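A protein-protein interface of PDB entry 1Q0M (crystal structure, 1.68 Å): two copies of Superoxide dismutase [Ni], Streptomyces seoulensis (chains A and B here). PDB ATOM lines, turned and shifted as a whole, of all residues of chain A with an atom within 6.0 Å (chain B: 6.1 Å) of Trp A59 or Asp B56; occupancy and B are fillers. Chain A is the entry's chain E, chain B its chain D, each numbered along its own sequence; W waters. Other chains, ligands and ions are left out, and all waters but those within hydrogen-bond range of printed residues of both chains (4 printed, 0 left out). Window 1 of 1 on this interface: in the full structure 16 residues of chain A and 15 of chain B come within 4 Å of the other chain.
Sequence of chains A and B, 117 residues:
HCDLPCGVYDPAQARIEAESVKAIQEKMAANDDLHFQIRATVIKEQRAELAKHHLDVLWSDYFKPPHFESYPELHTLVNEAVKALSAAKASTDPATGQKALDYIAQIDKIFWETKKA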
ATOM      1  N   HIS A  53      11.919  -5.959  -4.379  1.00  0.00           N
ATOM      2  CA  HIS A  53      11.344  -5.523  -5.647  1.00  0.00           C
ATOM      3  C   HIS A  53      12.241  -5.884  -6.826  1.00  0.00           C
ATOM      4  O   HIS A  53      11.763  -6.392  -7.844  1.00  0.00           O
ATOM      5  CB  HIS A  53      11.115  -4.011  -5.640  1.00  0.00           C
ATOM      6  CG  HIS A  53      10.706  -3.461  -6.972  1.00  0.00           C
ATOM      7  ND1 HIS A  53       9.505  -3.772  -7.568  1.00  0.00           N
ATOM      8  CD2 HIS A  53      11.355  -2.645  -7.835  1.00  0.00           C
ATOM      9  CE1 HIS A  53       9.431  -3.172  -8.744  1.00  0.00           C
ATOM     10  NE2 HIS A  53      10.540  -2.482  -8.930  1.00  0.00           N
ATOM     11  N   HIS A  54      13.536  -5.617  -6.691  1.00  0.00           N
ATOM     12  CA  HIS A  54      14.472  -5.916  -7.771  1.00  0.00           C
ATOM     13  C   HIS A  54      14.518  -7.411  -8.063  1.00  0.00           C
ATOM     14  O   HIS A  54      14.577  -7.815  -9.225  1.00  0.00           O
ATOM     15  CB  HIS A  54      15.875  -5.393  -7.441  1.00  0.00           C
ATOM     16  CG  HIS A  54      15.970  -3.898  -7.422  1.00  0.00           C
ATOM     17  ND1 HIS A  54      15.532  -3.112  -8.468  1.00  0.00           N
ATOM     18  CD2 HIS A  54      16.446  -3.045  -6.484  1.00  0.00           C
ATOM     19  CE1 HIS A  54      15.732  -1.839  -8.172  1.00  0.00           C
ATOM     20  NE2 HIS A  54      16.286  -1.772  -6.974  1.00  0.00           N
ATOM     21  N   LEU A  55      14.477  -8.235  -7.020  1.00  0.00           N
ATOM     22  CA  LEU A  55      14.494  -9.684  -7.225  1.00  0.00           C
ATOM     23  C   LEU A  55      13.176 -10.132  -7.852  1.00  0.00           C
ATOM     24  O   LEU A  55      13.155 -11.026  -8.704  1.00  0.00           O
ATOM     25  CB  LEU A  55      14.718 -10.418  -5.894  1.00  0.00           C
ATOM     26  CG  LEU A  55      16.095 -10.220  -5.250  1.00  0.00           C
ATOM     27  CD1 LEU A  55      16.178 -11.047  -3.979  1.00  0.00           C
ATOM     28  CD2 LEU A  55      17.196 -10.636  -6.226  1.00  0.00           C
ATOM     29  N   ASP A  56      12.073  -9.519  -7.432  1.00  0.00           N
ATOM     30  CA  ASP A  56      10.766  -9.866  -7.989  1.00  0.00           C
ATOM     31  C   ASP A  56      10.771  -9.585  -9.491  1.00  0.00           C
ATOM     32  O   ASP A  56      10.211 -10.350 -10.276  1.00  0.00           O
ATOM     33  CB  ASP A  56       9.647  -9.050  -7.329  1.00  0.00           C
ATOM     34  CG  ASP A  56       9.308  -9.538  -5.927  1.00  0.00           C
ATOM     35  OD1 ASP A  56       9.732 -10.653  -5.559  1.00  0.00           O
ATOM     36  OD2 ASP A  56       8.605  -8.803  -5.199  1.00  0.00           O
ATOM     37  N   VAL A  57      11.410  -8.485  -9.879  1.00  0.00           N
ATOM     38  CA  VAL A  57      11.489  -8.096 -11.287  1.00  0.00           C
ATOM     39  C   VAL A  57      12.296  -9.106 -12.099  1.00  0.00           C
ATOM     40  O   VAL A  57      11.917  -9.451 -13.218  1.00  0.00           O
ATOM     41  CB  VAL A  57      12.099  -6.678 -11.433  1.00  0.00           C
ATOM     42  CG1 VAL A  57      12.452  -6.388 -12.892  1.00  0.00           C
ATOM     43  CG2 VAL A  57      11.095  -5.646 -10.932  1.00  0.00           C
ATOM     44  N   LEU A  58      13.404  -9.583 -11.543  1.00  0.00           N
ATOM     45  CA  LEU A  58      14.215 -10.573 -12.252  1.00  0.00           C
ATOM     46  C   LEU A  58      13.374 -11.827 -12.458  1.00  0.00           C
ATOM     47  O   LEU A  58      13.341 -12.401 -13.542  1.00  0.00           O
ATOM     48  CB  LEU A  58      15.468 -10.929 -11.443  1.00  0.00           C
ATOM     49  CG  LEU A  58      16.536  -9.843 -11.299  1.00  0.00           C
ATOM     50  CD1 LEU A  58      17.658 -10.345 -10.407  1.00  0.00           C
ATOM     51  CD2 LEU A  58      17.076  -9.462 -12.680  1.00  0.00           C
ATOM     52  N   TRP A  59      12.680 -12.232 -11.400  1.00  0.00           N
ATOM     53  CA  TRP A  59      11.838 -13.424 -11.420  1.00  0.00           C
ATOM     54  C   TRP A  59      10.660 -13.332 -12.397  1.00  0.00           C
ATOM     55  O   TRP A  59      10.418 -14.254 -13.178  1.00  0.00           O
ATOM     56  CB  TRP A  59      11.319 -13.689  -9.995  1.00  0.00           C
ATOM     57  CG  TRP A  59      10.400 -14.869  -9.859  1.00  0.00           C
ATOM     58  CD1 TRP A  59      10.745 -16.190  -9.890  1.00  0.00           C
ATOM     59  CD2 TRP A  59       8.979 -14.829  -9.679  1.00  0.00           C
ATOM     60  NE1 TRP A  59       9.626 -16.975  -9.739  1.00  0.00           N
ATOM     61  CE2 TRP A  59       8.529 -16.166  -9.608  1.00  0.00           C
ATOM     62  CE3 TRP A  59       8.040 -13.792  -9.570  1.00  0.00           C
ATOM     63  CZ2 TRP A  59       7.177 -16.496  -9.434  1.00  0.00           C
ATOM     64  CZ3 TRP A  59       6.696 -14.118  -9.397  1.00  0.00           C
ATOM     65  CH2 TRP A  59       6.277 -15.463  -9.331  1.00  0.00           C
ATOM     66  N   SER A  60       9.938 -12.217 -12.367  1.00  0.00           N
ATOM     67  CA  SER A  60       8.771 -12.056 -13.224  1.00  0.00           C
ATOM     68  C   SER A  60       9.046 -11.626 -14.659  1.00  0.00           C
ATOM     69  O   SER A  60       8.386 -12.097 -15.583  1.00  0.00           O
ATOM     70  CB  SER A  60       7.798 -11.047 -12.608  1.00  0.00           C
ATOM     71  OG  SER A  60       8.360  -9.746 -12.602  1.00  0.00           O
ATOM     72  N   ASP A  61      10.018 -10.738 -14.833  1.00  0.00           N
ATOM     73  CA  ASP A  61      10.331 -10.176 -16.144  1.00  0.00           C
ATOM     74  C   ASP A  61      11.520 -10.759 -16.892  1.00  0.00           C
ATOM     75  O   ASP A  61      11.403 -11.103 -18.063  1.00  0.00           O
ATOM     76  CB  ASP A  61      10.533  -8.663 -16.007  1.00  0.00           C
ATOM     77  CG  ASP A  61       9.281  -7.938 -15.537  1.00  0.00           C
ATOM     78  OD1 ASP A  61       8.335  -8.600 -15.054  1.00  0.00           O
ATOM     79  OD2 ASP A  61       9.248  -6.692 -15.648  1.00  0.00           O
ATOM     80  N   TYR A  62      12.662 -10.884 -16.224  1.00  0.00           N
ATOM     81  CA  TYR A  62      13.844 -11.384 -16.908  1.00  0.00           C
ATOM     82  C   TYR A  62      13.819 -12.911 -17.151  1.00  0.00           C
ATOM     83  O   TYR A  62      13.918 -13.348 -18.303  1.00  0.00           O
ATOM     84  CB  TYR A  62      15.126 -11.029 -16.149  1.00  0.00           C
ATOM     85  CG  TYR A  62      16.313 -11.735 -16.790  1.00  0.00           C
ATOM     86  CD1 TYR A  62      16.809 -11.256 -17.999  1.00  0.00           C
ATOM     87  CD2 TYR A  62      16.904 -12.871 -16.235  1.00  0.00           C
ATOM     88  CE1 TYR A  62      17.841 -11.909 -18.662  1.00  0.00           C
ATOM     89  CE2 TYR A  62      17.936 -13.533 -16.891  1.00  0.00           C
ATOM     90  CZ  TYR A  62      18.395 -13.047 -18.106  1.00  0.00           C
ATOM     91  OH  TYR A  62      19.396 -13.715 -18.775  1.00  0.00           O
ATOM     92  N   PHE A  63      13.686 -13.701 -16.092  1.00  0.00           N
ATOM     93  CA  PHE A  63      13.683 -15.148 -16.256  1.00  0.00           C
ATOM     94  C   PHE A  63      12.464 -15.625 -17.029  1.00  0.00           C
ATOM     95  O   PHE A  63      11.330 -15.253 -16.723  1.00  0.00           O
ATOM     96  CB  PHE A  63      13.783 -15.838 -14.894  1.00  0.00           C
ATOM     97  CG  PHE A  63      15.143 -15.715 -14.263  1.00  0.00           C
ATOM     98  CD1 PHE A  63      16.270 -16.230 -14.906  1.00  0.00           C
ATOM     99  CD2 PHE A  63      15.304 -15.076 -13.039  1.00  0.00           C
ATOM    100  CE1 PHE A  63      17.539 -16.105 -14.339  1.00  0.00           C
ATOM    101  CE2 PHE A  63      16.567 -14.946 -12.461  1.00  0.00           C
ATOM    102  CZ  PHE A  63      17.690 -15.463 -13.113  1.00  0.00           C
ATOM    103  N   LYS A  64      12.722 -16.444 -18.045  1.00  0.00           N
ATOM    104  CA  LYS A  64      11.682 -16.978 -18.915  1.00  0.00           C
ATOM    105  C   LYS A  64      11.451 -18.465 -18.652  1.00  0.00           C
ATOM    106  O   LYS A  64      12.263 -19.122 -18.002  1.00  0.00           O
ATOM    107  CB  LYS A  64      12.090 -16.771 -20.377  1.00  0.00           C
ATOM    108  CG  LYS A  64      12.425 -15.332 -20.753  1.00  0.00           C
ATOM    109  CD  LYS A  64      11.219 -14.417 -20.620  1.00  0.00           C
ATOM    110  CE  LYS A  64      11.498 -13.040 -21.210  1.00  0.00           C
ATOM    111  NZ  LYS A  64      12.626 -12.343 -20.528  1.00  0.00           N
ATOM    112  N   PHE A  68      13.525 -21.565 -16.058  1.00  0.00           N
ATOM    113  CA  PHE A  68      13.023 -22.300 -14.904  1.00  0.00           C
ATOM    114  C   PHE A  68      13.104 -23.797 -15.155  1.00  0.00           C
ATOM    115  O   PHE A  68      13.218 -24.583 -14.220  1.00  0.00           O
ATOM    116  CB  PHE A  68      11.586 -21.880 -14.595  1.00  0.00           C
ATOM    117  CG  PHE A  68      11.462 -20.451 -14.144  1.00  0.00           C
ATOM    118  CD1 PHE A  68      12.062 -20.029 -12.961  1.00  0.00           C
ATOM    119  CD2 PHE A  68      10.764 -19.523 -14.915  1.00  0.00           C
ATOM    120  CE1 PHE A  68      11.965 -18.697 -12.546  1.00  0.00           C
ATOM    121  CE2 PHE A  68      10.660 -18.191 -14.513  1.00  0.00           C
ATOM    122  CZ  PHE A  68      11.265 -17.777 -13.326  1.00  0.00           C
ATOM    123  N   LEU A  74      15.399 -22.747  -9.331  1.00  0.00           N
ATOM    124  CA  LEU A  74      15.353 -21.290  -9.427  1.00  0.00           C
ATOM    125  C   LEU A  74      14.140 -20.627  -8.763  1.00  0.00           C
ATOM    126  O   LEU A  74      14.302 -19.631  -8.055  1.00  0.00           O
ATOM    127  CB  LEU A  74      15.459 -20.851 -10.893  1.00  0.00           C
ATOM    128  CG  LEU A  74      15.559 -19.338 -11.135  1.00  0.00           C
ATOM    129  CD1 LEU A  74      16.722 -18.743 -10.359  1.00  0.00           C
ATOM    130  CD2 LEU A  74      15.737 -19.078 -12.627  1.00  0.00           C
ATOM    131  N   HIS A  75      12.935 -21.153  -8.980  1.00  0.00           N
ATOM    132  CA  HIS A  75      11.754 -20.562  -8.343  1.00  0.00           C
ATOM    133  C   HIS A  75      11.953 -20.550  -6.832  1.00  0.00           C
ATOM    134  O   HIS A  75      11.765 -19.527  -6.173  1.00  0.00           O
ATOM    135  CB  HIS A  75      10.487 -21.365  -8.655  1.00  0.00           C
ATOM    136  CG  HIS A  75       9.881 -21.057  -9.988  1.00  0.00           C
ATOM    137  ND1 HIS A  75       9.468 -19.790 -10.345  1.00  0.00           N
ATOM    138  CD2 HIS A  75       9.587 -21.858 -11.040  1.00  0.00           C
ATOM    139  CE1 HIS A  75       8.946 -19.825 -11.558  1.00  0.00           C
ATOM    140  NE2 HIS A  75       9.007 -21.069 -12.003  1.00  0.00           N
ATOM    141  N   VAL A  78      14.755 -17.946  -5.652  1.00  0.00           N
ATOM    142  CA  VAL A  78      14.349 -16.549  -5.573  1.00  0.00           C
ATOM    143  C   VAL A  78      13.372 -16.338  -4.425  1.00  0.00           C
ATOM    144  O   VAL A  78      13.444 -15.325  -3.725  1.00  0.00           O
ATOM    145  CB  VAL A  78      13.700 -16.059  -6.884  1.00  0.00           C
ATOM    146  CG1 VAL A  78      13.321 -14.580  -6.752  1.00  0.00           C
ATOM    147  CG2 VAL A  78      14.674 -16.240  -8.039  1.00  0.00           C
ATOM    148  N   ALA B  51      -1.095  -4.553  -9.983  1.00  0.00           N
ATOM    149  CA  ALA B  51      -1.568  -5.935  -9.972  1.00  0.00           C
ATOM    150  C   ALA B  51      -0.380  -6.887  -9.815  1.00  0.00           C
ATOM    151  O   ALA B  51      -0.438  -7.850  -9.047  1.00  0.00           O
ATOM    152  CB  ALA B  51      -2.320  -6.234 -11.257  1.00  0.00           C
ATOM    153  N   LYS B  52       0.698  -6.615 -10.545  1.00  0.00           N
ATOM    154  CA  LYS B  52       1.897  -7.440 -10.468  1.00  0.00           C
ATOM    155  C   LYS B  52       2.467  -7.399  -9.053  1.00  0.00           C
ATOM    156  O   LYS B  52       2.875  -8.422  -8.509  1.00  0.00           O
ATOM    157  CB  LYS B  52       2.952  -6.952 -11.469  1.00  0.00           C
ATOM    158  CG  LYS B  52       2.598  -7.207 -12.931  1.00  0.00           C
ATOM    159  CD  LYS B  52       3.693  -6.687 -13.868  1.00  0.00           C
ATOM    160  CE  LYS B  52       4.998  -7.468 -13.711  1.00  0.00           C
ATOM    161  NZ  LYS B  52       6.134  -6.846 -14.459  1.00  0.00           N
ATOM    162  N   HIS B  53       2.481  -6.211  -8.457  1.00  0.00           N
ATOM    163  CA  HIS B  53       2.998  -6.049  -7.102  1.00  0.00           C
ATOM    164  C   HIS B  53       2.208  -6.897  -6.110  1.00  0.00           C
ATOM    165  O   HIS B  53       2.789  -7.594  -5.275  1.00  0.00           O
ATOM    166  CB  HIS B  53       2.929  -4.580  -6.673  1.00  0.00           C
ATOM    167  CG  HIS B  53       3.241  -4.364  -5.223  1.00  0.00           C
ATOM    168  ND1 HIS B  53       4.502  -4.544  -4.700  1.00  0.00           N
ATOM    169  CD2 HIS B  53       2.445  -4.022  -4.182  1.00  0.00           C
ATOM    170  CE1 HIS B  53       4.471  -4.322  -3.397  1.00  0.00           C
ATOM    171  NE2 HIS B  53       3.236  -4.005  -3.058  1.00  0.00           N
ATOM    172  N   HIS B  54       0.882  -6.838  -6.201  1.00  0.00           N
ATOM    173  CA  HIS B  54       0.042  -7.601  -5.287  1.00  0.00           C
ATOM    174  C   HIS B  54       0.279  -9.098  -5.414  1.00  0.00           C
ATOM    175  O   HIS B  54       0.317  -9.816  -4.414  1.00  0.00           O
ATOM    176  CB  HIS B  54      -1.435  -7.278  -5.515  1.00  0.00           C
ATOM    177  CG  HIS B  54      -1.809  -5.884  -5.123  1.00  0.00           C
ATOM    178  ND1 HIS B  54      -1.451  -5.336  -3.910  1.00  0.00           N
ATOM    179  CD2 HIS B  54      -2.512  -4.930  -5.777  1.00  0.00           C
ATOM    180  CE1 HIS B  54      -1.919  -4.101  -3.834  1.00  0.00           C
ATOM    181  NE2 HIS B  54      -2.566  -3.832  -4.953  1.00  0.00           N
ATOM    182  N   LEU B  55       0.440  -9.574  -6.642  1.00  0.00           N
ATOM    183  CA  LEU B  55       0.690 -10.994  -6.845  1.00  0.00           C
ATOM    184  C   LEU B  55       2.076 -11.368  -6.332  1.00  0.00           C
ATOM    185  O   LEU B  55       2.248 -12.430  -5.735  1.00  0.00           O
ATOM    186  CB  LEU B  55       0.552 -11.362  -8.326  1.00  0.00           C
ATOM    187  CG  LEU B  55      -0.868 -11.293  -8.902  1.00  0.00           C
ATOM    188  CD1 LEU B  55      -0.844 -11.700 -10.372  1.00  0.00           C
ATOM    189  CD2 LEU B  55      -1.795 -12.212  -8.111  1.00  0.00           C
ATOM    190  N   ASP B  56       3.063 -10.502  -6.564  1.00  0.00           N
ATOM    191  CA  ASP B  56       4.419 -10.762  -6.089  1.00  0.00           C
ATOM    192  C   ASP B  56       4.400 -10.921  -4.566  1.00  0.00           C
ATOM    193  O   ASP B  56       5.096 -11.771  -4.010  1.00  0.00           O
ATOM    194  CB  ASP B  56       5.371  -9.617  -6.456  1.00  0.00           C
ATOM    195  CG  ASP B  56       5.714  -9.581  -7.938  1.00  0.00           C
ATOM    196  OD1 ASP B  56       5.505 -10.596  -8.639  1.00  0.00           O
ATOM    197  OD2 ASP B  56       6.214  -8.532  -8.398  1.00  0.00           O
ATOM    198  N   VAL B  57       3.597 -10.096  -3.902  1.00  0.00           N
ATOM    199  CA  VAL B  57       3.479 -10.151  -2.446  1.00  0.00           C
ATOM    200  C   VAL B  57       2.877 -11.467  -1.961  1.00  0.00           C
ATOM    201  O   VAL B  57       3.320 -12.026  -0.953  1.00  0.00           O
ATOM    202  CB  VAL B  57       2.624  -8.973  -1.916  1.00  0.00           C
ATOM    203  CG1 VAL B  57       2.247  -9.202  -0.453  1.00  0.00           C
ATOM    204  CG2 VAL B  57       3.403  -7.678  -2.057  1.00  0.00           C
ATOM    205  N   LEU B  58       1.861 -11.963  -2.663  1.00  0.00           N
ATOM    206  CA  LEU B  58       1.245 -13.227  -2.271  1.00  0.00           C
ATOM    207  C   LEU B  58       2.296 -14.322  -2.380  1.00  0.00           C
ATOM    208  O   LEU B  58       2.436 -15.159  -1.495  1.00  0.00           O
ATOM    209  CB  LEU B  58       0.067 -13.572  -3.189  1.00  0.00           C
ATOM    210  CG  LEU B  58      -1.206 -12.738  -3.045  1.00  0.00           C
ATOM    211  CD1 LEU B  58      -2.241 -13.219  -4.054  1.00  0.00           C
ATOM    212  CD2 LEU B  58      -1.738 -12.866  -1.625  1.00  0.00           C
ATOM    213  N   TRP B  59       3.045 -14.289  -3.477  1.00  0.00           N
ATOM    214  CA  TRP B  59       4.088 -15.276  -3.742  1.00  0.00           C
ATOM    215  C   TRP B  59       5.272 -15.219  -2.770  1.00  0.00           C
ATOM    216  O   TRP B  59       5.729 -16.250  -2.274  1.00  0.00           O
ATOM    217  CB  TRP B  59       4.592 -15.088  -5.174  1.00  0.00           C
ATOM    218  CG  TRP B  59       5.705 -16.004  -5.572  1.00  0.00           C
ATOM    219  CD1 TRP B  59       5.604 -17.329  -5.892  1.00  0.00           C
ATOM    220  CD2 TRP B  59       7.086 -15.658  -5.710  1.00  0.00           C
ATOM    221  NE1 TRP B  59       6.842 -17.829  -6.226  1.00  0.00           N
ATOM    222  CE2 TRP B  59       7.770 -16.826  -6.121  1.00  0.00           C
ATOM    223  CE3 TRP B  59       7.817 -14.475  -5.527  1.00  0.00           C
ATOM    224  CZ2 TRP B  59       9.150 -16.845  -6.354  1.00  0.00           C
ATOM    225  CZ3 TRP B  59       9.191 -14.491  -5.757  1.00  0.00           C
ATOM    226  CH2 TRP B  59       9.843 -15.673  -6.168  1.00  0.00           C
ATOM    227  N   SER B  60       5.757 -14.014  -2.486  1.00  0.00           N
ATOM    228  CA  SER B  60       6.915 -13.848  -1.614  1.00  0.00           C
ATOM    229  C   SER B  60       6.613 -13.874  -0.124  1.00  0.00           C
ATOM    230  O   SER B  60       7.423 -14.363   0.660  1.00  0.00           O
ATOM    231  CB  SER B  60       7.634 -12.533  -1.935  1.00  0.00           C
ATOM    232  OG  SER B  60       6.838 -11.412  -1.563  1.00  0.00           O
ATOM    233  N   ASP B  61       5.452 -13.357   0.261  1.00  0.00           N
ATOM    234  CA  ASP B  61       5.095 -13.274   1.674  1.00  0.00           C
ATOM    235  C   ASP B  61       4.058 -14.260   2.200  1.00  0.00           C
ATOM    236  O   ASP B  61       4.289 -14.907   3.219  1.00  0.00           O
ATOM    237  CB  ASP B  61       4.617 -11.855   2.002  1.00  0.00           C
ATOM    238  CG  ASP B  61       5.677 -10.801   1.746  1.00  0.00           C
ATOM    239  OD1 ASP B  61       6.741 -11.130   1.180  1.00  0.00           O
ATOM    240  OD2 ASP B  61       5.434  -9.632   2.110  1.00  0.00           O
ATOM    241  N   HIS B  75       4.302 -22.011  -8.233  1.00  0.00           N
ATOM    242  CA  HIS B  75       5.334 -21.063  -8.657  1.00  0.00           C
ATOM    243  C   HIS B  75       5.065 -20.617 -10.091  1.00  0.00           C
ATOM    244  O   HIS B  75       5.049 -19.423 -10.394  1.00  0.00           O
ATOM    245  CB  HIS B  75       6.729 -21.692  -8.618  1.00  0.00           C
ATOM    246  CG  HIS B  75       7.330 -21.776  -7.251  1.00  0.00           C
ATOM    247  ND1 HIS B  75       7.488 -20.677  -6.434  1.00  0.00           N
ATOM    248  CD2 HIS B  75       7.867 -22.823  -6.579  1.00  0.00           C
ATOM    249  CE1 HIS B  75       8.099 -21.042  -5.321  1.00  0.00           C
ATOM    250  NE2 HIS B  75       8.339 -22.341  -5.384  1.00  0.00           N
ATOM    251  N   THR B  76       4.866 -21.593 -10.972  1.00  0.00           N
ATOM    252  CA  THR B  76       4.618 -21.315 -12.377  1.00  0.00           C
ATOM    253  C   THR B  76       3.330 -20.528 -12.584  1.00  0.00           C
ATOM    254  O   THR B  76       3.275 -19.629 -13.420  1.00  0.00           O
ATOM    255  CB  THR B  76       4.554 -22.622 -13.192  1.00  0.00           C
ATOM    256  OG1 THR B  76       5.833 -23.262 -13.146  1.00  0.00           O
ATOM    257  CG2 THR B  76       4.183 -22.336 -14.640  1.00  0.00           C
ATOM    258  N   VAL B  78       1.806 -18.320 -10.533  1.00  0.00           N
ATOM    259  CA  VAL B  78       1.974 -16.906 -10.218  1.00  0.00           C
ATOM    260  C   VAL B  78       2.903 -16.246 -11.233  1.00  0.00           C
ATOM    261  O   VAL B  78       2.666 -15.116 -11.651  1.00  0.00           O
ATOM    262  CB  VAL B  78       2.532 -16.693  -8.794  1.00  0.00           C
ATOM    263  CG1 VAL B  78       2.636 -15.185  -8.496  1.00  0.00           C
ATOM    264  CG2 VAL B  78       1.613 -17.363  -7.772  1.00  0.00           C
ATOM    265  N   ASN B  79       3.949 -16.958 -11.645  1.00  0.00           N
ATOM    266  CA  ASN B  79       4.886 -16.401 -12.613  1.00  0.00           C
ATOM    267  C   ASN B  79       4.193 -16.127 -13.951  1.00  0.00           C
ATOM    268  O   ASN B  79       4.438 -15.097 -14.582  1.00  0.00           O
ATOM    269  CB  ASN B  79       6.078 -17.343 -12.810  1.00  0.00           C
ATOM    270  CG  ASN B  79       7.236 -16.668 -13.527  1.00  0.00           C
ATOM    271  OD1 ASN B  79       7.386 -16.785 -14.742  1.00  0.00           O
ATOM    272  ND2 ASN B  79       8.051 -15.938 -12.772  1.00  0.00           N
ATOM    273  N   GLU B  80       3.316 -17.031 -14.377  1.00  0.00           N
ATOM    274  CA  GLU B  80       2.607 -16.824 -15.635  1.00  0.00           C
ATOM    275  C   GLU B  80       1.587 -15.695 -15.496  1.00  0.00           C
ATOM    276  O   GLU B  80       1.315 -14.972 -16.452  1.00  0.00           O
ATOM    277  CB  GLU B  80       1.916 -18.113 -16.086  1.00  0.00           C
ATOM    278  CG  GLU B  80       2.894 -19.237 -16.367  1.00  0.00           C
ATOM    279  CD  GLU B  80       2.232 -20.457 -16.977  1.00  0.00           C
ATOM    280  OE1 GLU B  80       1.096 -20.781 -16.576  1.00  0.00           O
ATOM    281  OE2 GLU B  80       2.857 -21.098 -17.849  1.00  0.00           O
ATOM    282  N   VAL B  82       1.890 -12.940 -13.571  1.00  0.00           N
ATOM    283  CA  VAL B  82       2.574 -11.653 -13.650  1.00  0.00           C
ATOM    284  C   VAL B  82       3.060 -11.397 -15.074  1.00  0.00           C
ATOM    285  O   VAL B  82       3.059 -10.261 -15.534  1.00  0.00           O
ATOM    286  CB  VAL B  82       3.756 -11.550 -12.649  1.00  0.00           C
ATOM    287  CG1 VAL B  82       3.214 -11.572 -11.219  1.00  0.00           C
ATOM    288  CG2 VAL B  82       4.743 -12.685 -12.863  1.00  0.00           C
ATOM    289  N   LYS B  83       3.453 -12.452 -15.784  1.00  0.00           N
ATOM    290  CA  LYS B  83       3.883 -12.277 -17.166  1.00  0.00           C
ATOM    291  C   LYS B  83       2.677 -11.891 -18.027  1.00  0.00           C
ATOM    292  O   LYS B  83       2.808 -11.139 -19.004  1.00  0.00           O
ATOM    293  CB  LYS B  83       4.533 -13.559 -17.700  1.00  0.00           C
ATOM    294  CG  LYS B  83       5.979 -13.740 -17.255  1.00  0.00           C
ATOM    295  CD  LYS B  83       6.537 -15.088 -17.699  1.00  0.00           C
ATOM    296  CE  LYS B  83       8.058 -15.117 -17.609  1.00  0.00           C
ATOM    297  NZ  LYS B  83       8.556 -14.775 -16.252  1.00  0.00           N
HETATM  298  O   HOH W   1       7.018  -8.108 -10.867  1.00  0.00           O
HETATM  299  O   HOH W   2       7.186  -6.335  -6.459  1.00  0.00           O
HETATM  300  O   HOH W   3       7.829  -9.116  -2.716  1.00  0.00           O
HETATM  301  O   HOH W   4       7.865 -21.869 -14.509  1.00  0.00           O
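Trp B59 touches its own counterpart, Trp A59. Trp A59 touches His B75, and with the chains exchanged His A75 touches Trp B59. Trp A59 touches Val B78, and with the chains exchanged Val A78 touches Trp B59. His B75 touches its own counterpart, His A75. 11 positions are printed for both chains. Of the 18 pairs that touch across the chains among the printed residues, 9 have their exchanged pair printed and touching as well.
Of the 18 printed residues of chain B, 8 touch a printed residue of chain A. Hydrophobic or aromatic side chains of chain B within 4 Å of the printed part of chain A: Trp B59, His B75, Val B78 and Val B82. Along chain B the printed residues that touch a printed residue of chain A span positions 52 to 83. Of the 16 printed residues of chain A, 8 touch a printed residue of chain B. Hydrophobic or aromatic side chains of chain A that line the printed part of chain B: Trp A59, Phe A68, His A75 and Val A78. Among the printed residues, 18 pairs touch across the chains. Among the printed residues, Asp or Glu carboxylates within 4 Å of a Lys or Arg side-chain nitrogen of the other chain: Asp A61 with Lys B52.
Printed residues of chain B within 4 Å of Asp A56: Asp B56 and Trp B59. Printed residues of chain B within 4 Å of Asp A61: Lys B52 (2.9 Å). Tyr A62 touches none of the printed residues of chain B. Of chain A, only Asp A56 (3.6 Å) and Trp A59 (3.8 Å) come within 4 Å of Asp B56. Of the printed residues of chain A, His B75 touches Trp A59 (3.7 Å) and His A75 (3.5 Å). Printed residues of chain A within 4 Å of Lys B83: Trp A59, Ser A60 and Phe A63. The nearest residue of chain A that does not touch Asp B56 is Ser A60 (4.6 Å). The nearest printed residue of chain A that does not touch Lys B83 is Lys A64 (4.3 Å).
The side-chain carboxylate (OD1) of Asp A61 is in salt-bridge range of the side-chain amino group (NZ) of Lys B52, at 2.9 Å. The side-chain amino group (NZ) of Lys B83 sits at hydrogen-bond distance from the backbone carbonyl oxygen (O) of Ser A60, at 2.8 Å. The side-chain amino group (NZ) of Lys B83 is in hydrogen-bond range of the backbone carbonyl oxygen (O) of Phe A63 (2.9 Å). The side-chain amide nitrogen (ND2) of Asn B79 lies within hydrogen-bond range of the backbone carbonyl oxygen (O) of Trp A59.
O of Asp A56 is in hydrogen-bond range of OG of Ser A60 (3.0 Å). O of Asp A61 is in hydrogen-bond range of NZ of Lys A64, 3.0 Å away. OD1 of Asn B79 lies within hydrogen-bond range of NZ of Lys B83. The side-chain hydroxyl (OG) of Ser A60 sits at hydrogen-bond distance from the side-chain carboxylate (OD1) of Asp A61.
Among the printed residues, pairs that only touch across the chains: Trp A59 with Trp B59, Ser A60 with Val B82, His A75 with His B75, Asp A56 with Asp B56, Phe A68 with Asn B79, Trp A59 with Lys B83, Val A78 with Trp B59, Trp A59 with His B75, Trp A59 with Val B78, His A75 with Trp B59, Trp A59 with Asp B56, Asp A56 with Trp B59, Ser A60 with Asn B79 and His A75 with Asn B79.
Water W3 lies within hydrogen-bond range of OD2 of Asp A56 (2.6 Å) and OG of Ser B60 (2.8 Å). Water W1 bridges the side-chain carboxylate (OD2) of Asp B56 and the side-chain hydroxyl (OG) of Ser A60. Water W4 bridges OG1 of Thr B76 (2.8 Å) and NE2 of His A75 (2.9 Å). Water W2 bridges the side-chain carboxylate (OD2) of Asp B56 (3.1 Å) and the side-chain carboxylate (OD2) of Asp A56 (3.1 Å).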
